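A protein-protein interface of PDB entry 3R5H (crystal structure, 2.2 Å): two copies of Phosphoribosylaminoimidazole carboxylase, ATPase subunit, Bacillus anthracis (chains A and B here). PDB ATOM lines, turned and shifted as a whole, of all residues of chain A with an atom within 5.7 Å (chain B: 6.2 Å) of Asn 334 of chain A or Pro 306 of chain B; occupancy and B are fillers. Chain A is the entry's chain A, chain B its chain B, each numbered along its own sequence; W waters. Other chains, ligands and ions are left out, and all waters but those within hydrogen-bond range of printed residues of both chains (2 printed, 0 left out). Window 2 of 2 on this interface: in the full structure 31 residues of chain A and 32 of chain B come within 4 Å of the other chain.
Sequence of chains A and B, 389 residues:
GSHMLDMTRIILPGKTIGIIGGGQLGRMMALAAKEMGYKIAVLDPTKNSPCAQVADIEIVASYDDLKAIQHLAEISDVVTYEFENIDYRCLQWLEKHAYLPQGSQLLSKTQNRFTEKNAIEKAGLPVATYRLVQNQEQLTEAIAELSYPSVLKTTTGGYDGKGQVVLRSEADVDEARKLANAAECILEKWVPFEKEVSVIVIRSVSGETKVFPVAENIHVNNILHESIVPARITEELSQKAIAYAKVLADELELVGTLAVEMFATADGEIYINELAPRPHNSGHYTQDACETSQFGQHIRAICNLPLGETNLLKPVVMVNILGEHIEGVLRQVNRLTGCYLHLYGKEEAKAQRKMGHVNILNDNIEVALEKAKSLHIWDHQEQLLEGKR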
ATOM      1  N   LEU A 330      -2.438  20.028   4.505  1.00  0.00           N
ATOM      2  CA  LEU A 330      -2.304  19.148   5.689  1.00  0.00           C
ATOM      3  C   LEU A 330      -2.084  19.954   6.964  1.00  0.00           C
ATOM      4  O   LEU A 330      -2.611  19.618   8.017  1.00  0.00           O
ATOM      5  CB  LEU A 330      -1.151  18.155   5.501  1.00  0.00           C
ATOM      6  CG  LEU A 330      -1.281  17.230   4.288  1.00  0.00           C
ATOM      7  CD1 LEU A 330      -0.096  16.269   4.172  1.00  0.00           C
ATOM      8  CD2 LEU A 330      -2.616  16.449   4.332  1.00  0.00           C
ATOM      9  N   ARG A 331      -1.314  21.031   6.839  1.00  0.00           N
ATOM     10  CA  ARG A 331      -0.953  21.891   7.952  1.00  0.00           C
ATOM     11  C   ARG A 331      -2.160  22.720   8.403  1.00  0.00           C
ATOM     12  O   ARG A 331      -2.280  23.068   9.588  1.00  0.00           O
ATOM     13  CB  ARG A 331       0.196  22.810   7.518  1.00  0.00           C
ATOM     14  CG  ARG A 331       0.930  23.539   8.640  1.00  0.00           C
ATOM     15  CD  ARG A 331       1.949  24.576   8.101  1.00  0.00           C
ATOM     16  NE  ARG A 331       2.643  24.117   6.890  1.00  0.00           N
ATOM     17  CZ  ARG A 331       2.665  24.781   5.731  1.00  0.00           C
ATOM     18  NH1 ARG A 331       2.059  25.967   5.606  1.00  0.00           N
ATOM     19  NH2 ARG A 331       3.314  24.263   4.695  1.00  0.00           N
ATOM     20  N   GLN A 332      -3.046  23.024   7.454  1.00  0.00           N
ATOM     21  CA  GLN A 332      -4.205  23.885   7.688  1.00  0.00           C
ATOM     22  C   GLN A 332      -5.477  23.084   7.850  1.00  0.00           C
ATOM     23  O   GLN A 332      -6.575  23.654   7.862  1.00  0.00           O
ATOM     24  CB  GLN A 332      -4.402  24.870   6.528  1.00  0.00           C
ATOM     25  CG  GLN A 332      -3.276  25.891   6.304  1.00  0.00           C
ATOM     26  CD  GLN A 332      -3.211  26.936   7.385  1.00  0.00           C
ATOM     27  OE1 GLN A 332      -3.912  27.958   7.338  1.00  0.00           O
ATOM     28  NE2 GLN A 332      -2.349  26.700   8.367  1.00  0.00           N
ATOM     29  N   VAL A 333      -5.336  21.768   7.981  1.00  0.00           N
ATOM     30  CA  VAL A 333      -6.493  20.872   8.029  1.00  0.00           C
ATOM     31  C   VAL A 333      -7.565  21.260   9.068  1.00  0.00           C
ATOM     32  O   VAL A 333      -8.752  21.206   8.791  1.00  0.00           O
ATOM     33  CB  VAL A 333      -6.065  19.390   8.141  1.00  0.00           C
ATOM     34  CG1 VAL A 333      -5.649  19.017   9.575  1.00  0.00           C
ATOM     35  CG2 VAL A 333      -7.170  18.491   7.645  1.00  0.00           C
ATOM     36  N   ASN A 334      -7.132  21.712  10.239  1.00  0.00           N
ATOM     37  CA  ASN A 334      -8.038  22.165  11.292  1.00  0.00           C
ATOM     38  C   ASN A 334      -8.846  23.400  10.911  1.00  0.00           C
ATOM     39  O   ASN A 334      -9.768  23.797  11.634  1.00  0.00           O
ATOM     40  CB  ASN A 334      -7.251  22.441  12.569  1.00  0.00           C
ATOM     41  CG  ASN A 334      -6.141  23.453  12.350  1.00  0.00           C
ATOM     42  OD1 ASN A 334      -5.178  23.208  11.588  1.00  0.00           O
ATOM     43  ND2 ASN A 334      -6.278  24.607  12.984  1.00  0.00           N
ATOM     44  N   ARG A 335      -8.525  24.010   9.774  1.00  0.00           N
ATOM     45  CA  ARG A 335      -9.249  25.200   9.355  1.00  0.00           C
ATOM     46  C   ARG A 335     -10.245  24.941   8.200  1.00  0.00           C
ATOM     47  O   ARG A 335     -10.844  25.879   7.657  1.00  0.00           O
ATOM     48  CB  ARG A 335      -8.274  26.339   9.033  1.00  0.00           C
ATOM     49  CG  ARG A 335      -7.348  26.720  10.204  1.00  0.00           C
ATOM     50  CD  ARG A 335      -7.312  28.230  10.418  1.00  0.00           C
ATOM     51  NE  ARG A 335      -6.796  28.952   9.247  1.00  0.00           N
ATOM     52  CZ  ARG A 335      -5.702  29.715   9.238  1.00  0.00           C
ATOM     53  NH1 ARG A 335      -4.979  29.891  10.343  1.00  0.00           N
ATOM     54  NH2 ARG A 335      -5.334  30.318   8.111  1.00  0.00           N
ATOM     55  N   LEU A 336     -10.453  23.668   7.871  1.00  0.00           N
ATOM     56  CA  LEU A 336     -11.257  23.299   6.709  1.00  0.00           C
ATOM     57  C   LEU A 336     -12.767  23.199   6.952  1.00  0.00           C
ATOM     58  O   LEU A 336     -13.467  22.414   6.298  1.00  0.00           O
ATOM     59  CB  LEU A 336     -10.703  22.035   6.050  1.00  0.00           C
ATOM     60  CG  LEU A 336      -9.306  22.152   5.419  1.00  0.00           C
ATOM     61  CD1 LEU A 336      -8.895  20.836   4.759  1.00  0.00           C
ATOM     62  CD2 LEU A 336      -9.235  23.289   4.401  1.00  0.00           C
ATOM     63  N   THR A 337     -13.275  24.017   7.871  1.00  0.00           N
ATOM     64  CA  THR A 337     -14.724  24.149   8.070  1.00  0.00           C
ATOM     65  C   THR A 337     -15.418  24.648   6.780  1.00  0.00           C
ATOM     66  O   THR A 337     -14.898  25.512   6.074  1.00  0.00           O
ATOM     67  CB  THR A 337     -15.053  25.045   9.295  1.00  0.00           C
ATOM     68  OG1 THR A 337     -16.455  25.343   9.325  1.00  0.00           O
ATOM     69  CG2 THR A 337     -14.294  26.340   9.235  1.00  0.00           C
ATOM     70  N   ILE B  10      -4.656  14.466  15.571  1.00  0.00           N
ATOM     71  CA  ILE B  10      -5.252  14.503  14.247  1.00  0.00           C
ATOM     72  C   ILE B  10      -4.668  13.373  13.410  1.00  0.00           C
ATOM     73  O   ILE B  10      -3.447  13.206  13.353  1.00  0.00           O
ATOM     74  CB  ILE B  10      -5.045  15.898  13.584  1.00  0.00           C
ATOM     75  CG1 ILE B  10      -5.895  16.950  14.310  1.00  0.00           C
ATOM     76  CG2 ILE B  10      -5.394  15.867  12.070  1.00  0.00           C
ATOM     77  CD1 ILE B  10      -5.635  18.398  13.891  1.00  0.00           C
ATOM     78  N   GLU B 208     -16.289  18.870  18.938  1.00  0.00           N
ATOM     79  CA  GLU B 208     -17.198  19.548  18.004  1.00  0.00           C
ATOM     80  C   GLU B 208     -18.400  18.641  17.736  1.00  0.00           C
ATOM     81  O   GLU B 208     -18.223  17.442  17.531  1.00  0.00           O
ATOM     82  CB  GLU B 208     -16.464  19.887  16.685  1.00  0.00           C
ATOM     83  CG  GLU B 208     -17.305  20.655  15.679  1.00  0.00           C
ATOM     84  CD  GLU B 208     -16.598  20.874  14.337  1.00  0.00           C
ATOM     85  OE1 GLU B 208     -15.549  20.225  14.062  1.00  0.00           O
ATOM     86  OE2 GLU B 208     -17.113  21.707  13.557  1.00  0.00           O
ATOM     87  N   GLN B 297     -18.846  12.201   7.972  1.00  0.00           N
ATOM     88  CA  GLN B 297     -18.826  12.744   9.336  1.00  0.00           C
ATOM     89  C   GLN B 297     -18.125  11.807  10.320  1.00  0.00           C
ATOM     90  O   GLN B 297     -17.327  12.245  11.139  1.00  0.00           O
ATOM     91  CB  GLN B 297     -20.245  13.016   9.840  1.00  0.00           C
ATOM     92  CG  GLN B 297     -20.942  14.149   9.173  1.00  0.00           C
ATOM     93  CD  GLN B 297     -20.405  15.515   9.587  1.00  0.00           C
ATOM     94  OE1 GLN B 297     -19.198  15.733   9.652  1.00  0.00           O
ATOM     95  NE2 GLN B 297     -21.310  16.447   9.840  1.00  0.00           N
ATOM     96  N   ARG B 300     -14.449  11.975   9.735  1.00  0.00           N
ATOM     97  CA  ARG B 300     -13.968  13.265  10.226  1.00  0.00           C
ATOM     98  C   ARG B 300     -13.900  13.267  11.757  1.00  0.00           C
ATOM     99  O   ARG B 300     -12.936  13.782  12.334  1.00  0.00           O
ATOM    100  CB  ARG B 300     -14.839  14.417   9.721  1.00  0.00           C
ATOM    101  CG  ARG B 300     -14.630  14.773   8.244  1.00  0.00           C
ATOM    102  CD  ARG B 300     -15.761  15.650   7.692  1.00  0.00           C
ATOM    103  NE  ARG B 300     -15.416  16.189   6.366  1.00  0.00           N
ATOM    104  CZ  ARG B 300     -15.624  15.555   5.204  1.00  0.00           C
ATOM    105  NH1 ARG B 300     -16.190  14.351   5.168  1.00  0.00           N
ATOM    106  NH2 ARG B 300     -15.264  16.125   4.058  1.00  0.00           N
ATOM    107  N   ASN B 304     -10.416  13.548  13.734  1.00  0.00           N
ATOM    108  CA  ASN B 304     -10.389  14.871  14.342  1.00  0.00           C
ATOM    109  C   ASN B 304     -10.238  16.026  13.340  1.00  0.00           C
ATOM    110  O   ASN B 304      -9.580  17.039  13.626  1.00  0.00           O
ATOM    111  CB  ASN B 304      -9.328  14.946  15.457  1.00  0.00           C
ATOM    112  CG  ASN B 304      -9.648  16.006  16.476  1.00  0.00           C
ATOM    113  OD1 ASN B 304     -10.779  16.483  16.536  1.00  0.00           O
ATOM    114  ND2 ASN B 304      -8.656  16.400  17.265  1.00  0.00           N
ATOM    115  N   LEU B 305     -10.847  15.873  12.166  1.00  0.00           N
ATOM    116  CA  LEU B 305     -10.938  16.976  11.218  1.00  0.00           C
ATOM    117  C   LEU B 305     -12.142  17.841  11.611  1.00  0.00           C
ATOM    118  O   LEU B 305     -12.997  17.398  12.388  1.00  0.00           O
ATOM    119  CB  LEU B 305     -11.102  16.436   9.783  1.00  0.00           C
ATOM    120  CG  LEU B 305     -10.165  15.275   9.416  1.00  0.00           C
ATOM    121  CD1 LEU B 305     -10.489  14.649   8.055  1.00  0.00           C
ATOM    122  CD2 LEU B 305      -8.697  15.698   9.488  1.00  0.00           C
ATOM    123  N   PRO B 306     -12.211  19.087  11.109  1.00  0.00           N
ATOM    124  CA  PRO B 306     -13.472  19.789  11.335  1.00  0.00           C
ATOM    125  C   PRO B 306     -14.625  18.989  10.726  1.00  0.00           C
ATOM    126  O   PRO B 306     -14.452  18.323   9.686  1.00  0.00           O
ATOM    127  CB  PRO B 306     -13.284  21.108  10.582  1.00  0.00           C
ATOM    128  CG  PRO B 306     -11.798  21.307  10.532  1.00  0.00           C
ATOM    129  CD  PRO B 306     -11.199  19.937  10.450  1.00  0.00           C
ATOM    130  N   LEU B 307     -15.786  19.025  11.364  1.00  0.00           N
ATOM    131  CA  LEU B 307     -16.928  18.295  10.842  1.00  0.00           C
ATOM    132  C   LEU B 307     -17.532  19.038   9.660  1.00  0.00           C
ATOM    133  O   LEU B 307     -17.386  20.258   9.564  1.00  0.00           O
ATOM    134  CB  LEU B 307     -17.978  18.059  11.943  1.00  0.00           C
ATOM    135  CG  LEU B 307     -17.555  17.180  13.130  1.00  0.00           C
ATOM    136  CD1 LEU B 307     -18.742  16.947  14.093  1.00  0.00           C
ATOM    137  CD2 LEU B 307     -16.935  15.835  12.671  1.00  0.00           C
ATOM    138  N   GLY B 308     -18.186  18.304   8.758  1.00  0.00           N
ATOM    139  CA  GLY B 308     -18.910  18.929   7.665  1.00  0.00           C
ATOM    140  C   GLY B 308     -20.268  19.420   8.153  1.00  0.00           C
ATOM    141  O   GLY B 308     -20.658  19.129   9.286  1.00  0.00           O
HETATM  142  O   HOH W   1     -16.709  22.436  11.253  1.00  0.00           O
HETATM  143  O   HOH W   2     -18.187  22.549   8.141  1.00  0.00           O
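Of the 8 printed residues of chain A, 4 touch a printed residue of chain B.
Hydrophobic or aromatic side chains of chain A within 4 Å of the printed part of chain B: Val 333.
Of the 9 printed residues of chain B, 2 touch a printed residue of chain A.
Hydrophobic or aromatic side chains of chain B within 4 Å of the printed part of chain A: Leu 305 and Pro 306.
Along chain B the printed residues that touch a printed residue of chain A span positions 305 to 306.
Of the printed residues of chain B, Val 333 of chain A touches Leu 305 (3.7 Å) and Pro 306 (3.2 Å).
Asn 334 of chain A touches just one residue of chain B: Pro 306.
Of the printed residues of chain B, Leu 336 of chain A touches Pro 306 (3.8 Å).
Of the printed residues of chain B, Thr 337 of chain A touches Pro 306 (3.98 Å).
Of the printed residues of chain A, Leu 305 of chain B touches Val 333 (3.7 Å).
Pro 306 of chain B touches four residues of chain A.
No position is printed for both chains.
Val 333 of chain A touches Leu 305 of chain B (CG2 to CD2, 3.7 Å).
Val 333 of chain A touches Pro 306 of chain B.
Pro 306 of chain B touches Asn 334 of chain A.
Leu 336 of chain A touches Pro 306 of chain B.
CB of Pro 306 of chain B touches N of Thr 337 of chain A, 3.98 Å away.
Water W1 lies within hydrogen-bond range of the side-chain carboxylate (OE2) of Glu 208 of chain B, the backbone carbonyl oxygen (O) of Leu 307 of chain B and the side-chain hydroxyl (OG1) of Thr 337 of chain A.
Water W2 lies within hydrogen-bond range of the backbone carbonyl oxygen of Leu 307 of chain B (2.8 Å) and the side-chain hydroxyl of Thr 337 of chain A (3.5 Å).
N of Leu 305 of chain B is in hydrogen-bond range of O of Arg 300 of chain B, 3.0 Å away.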
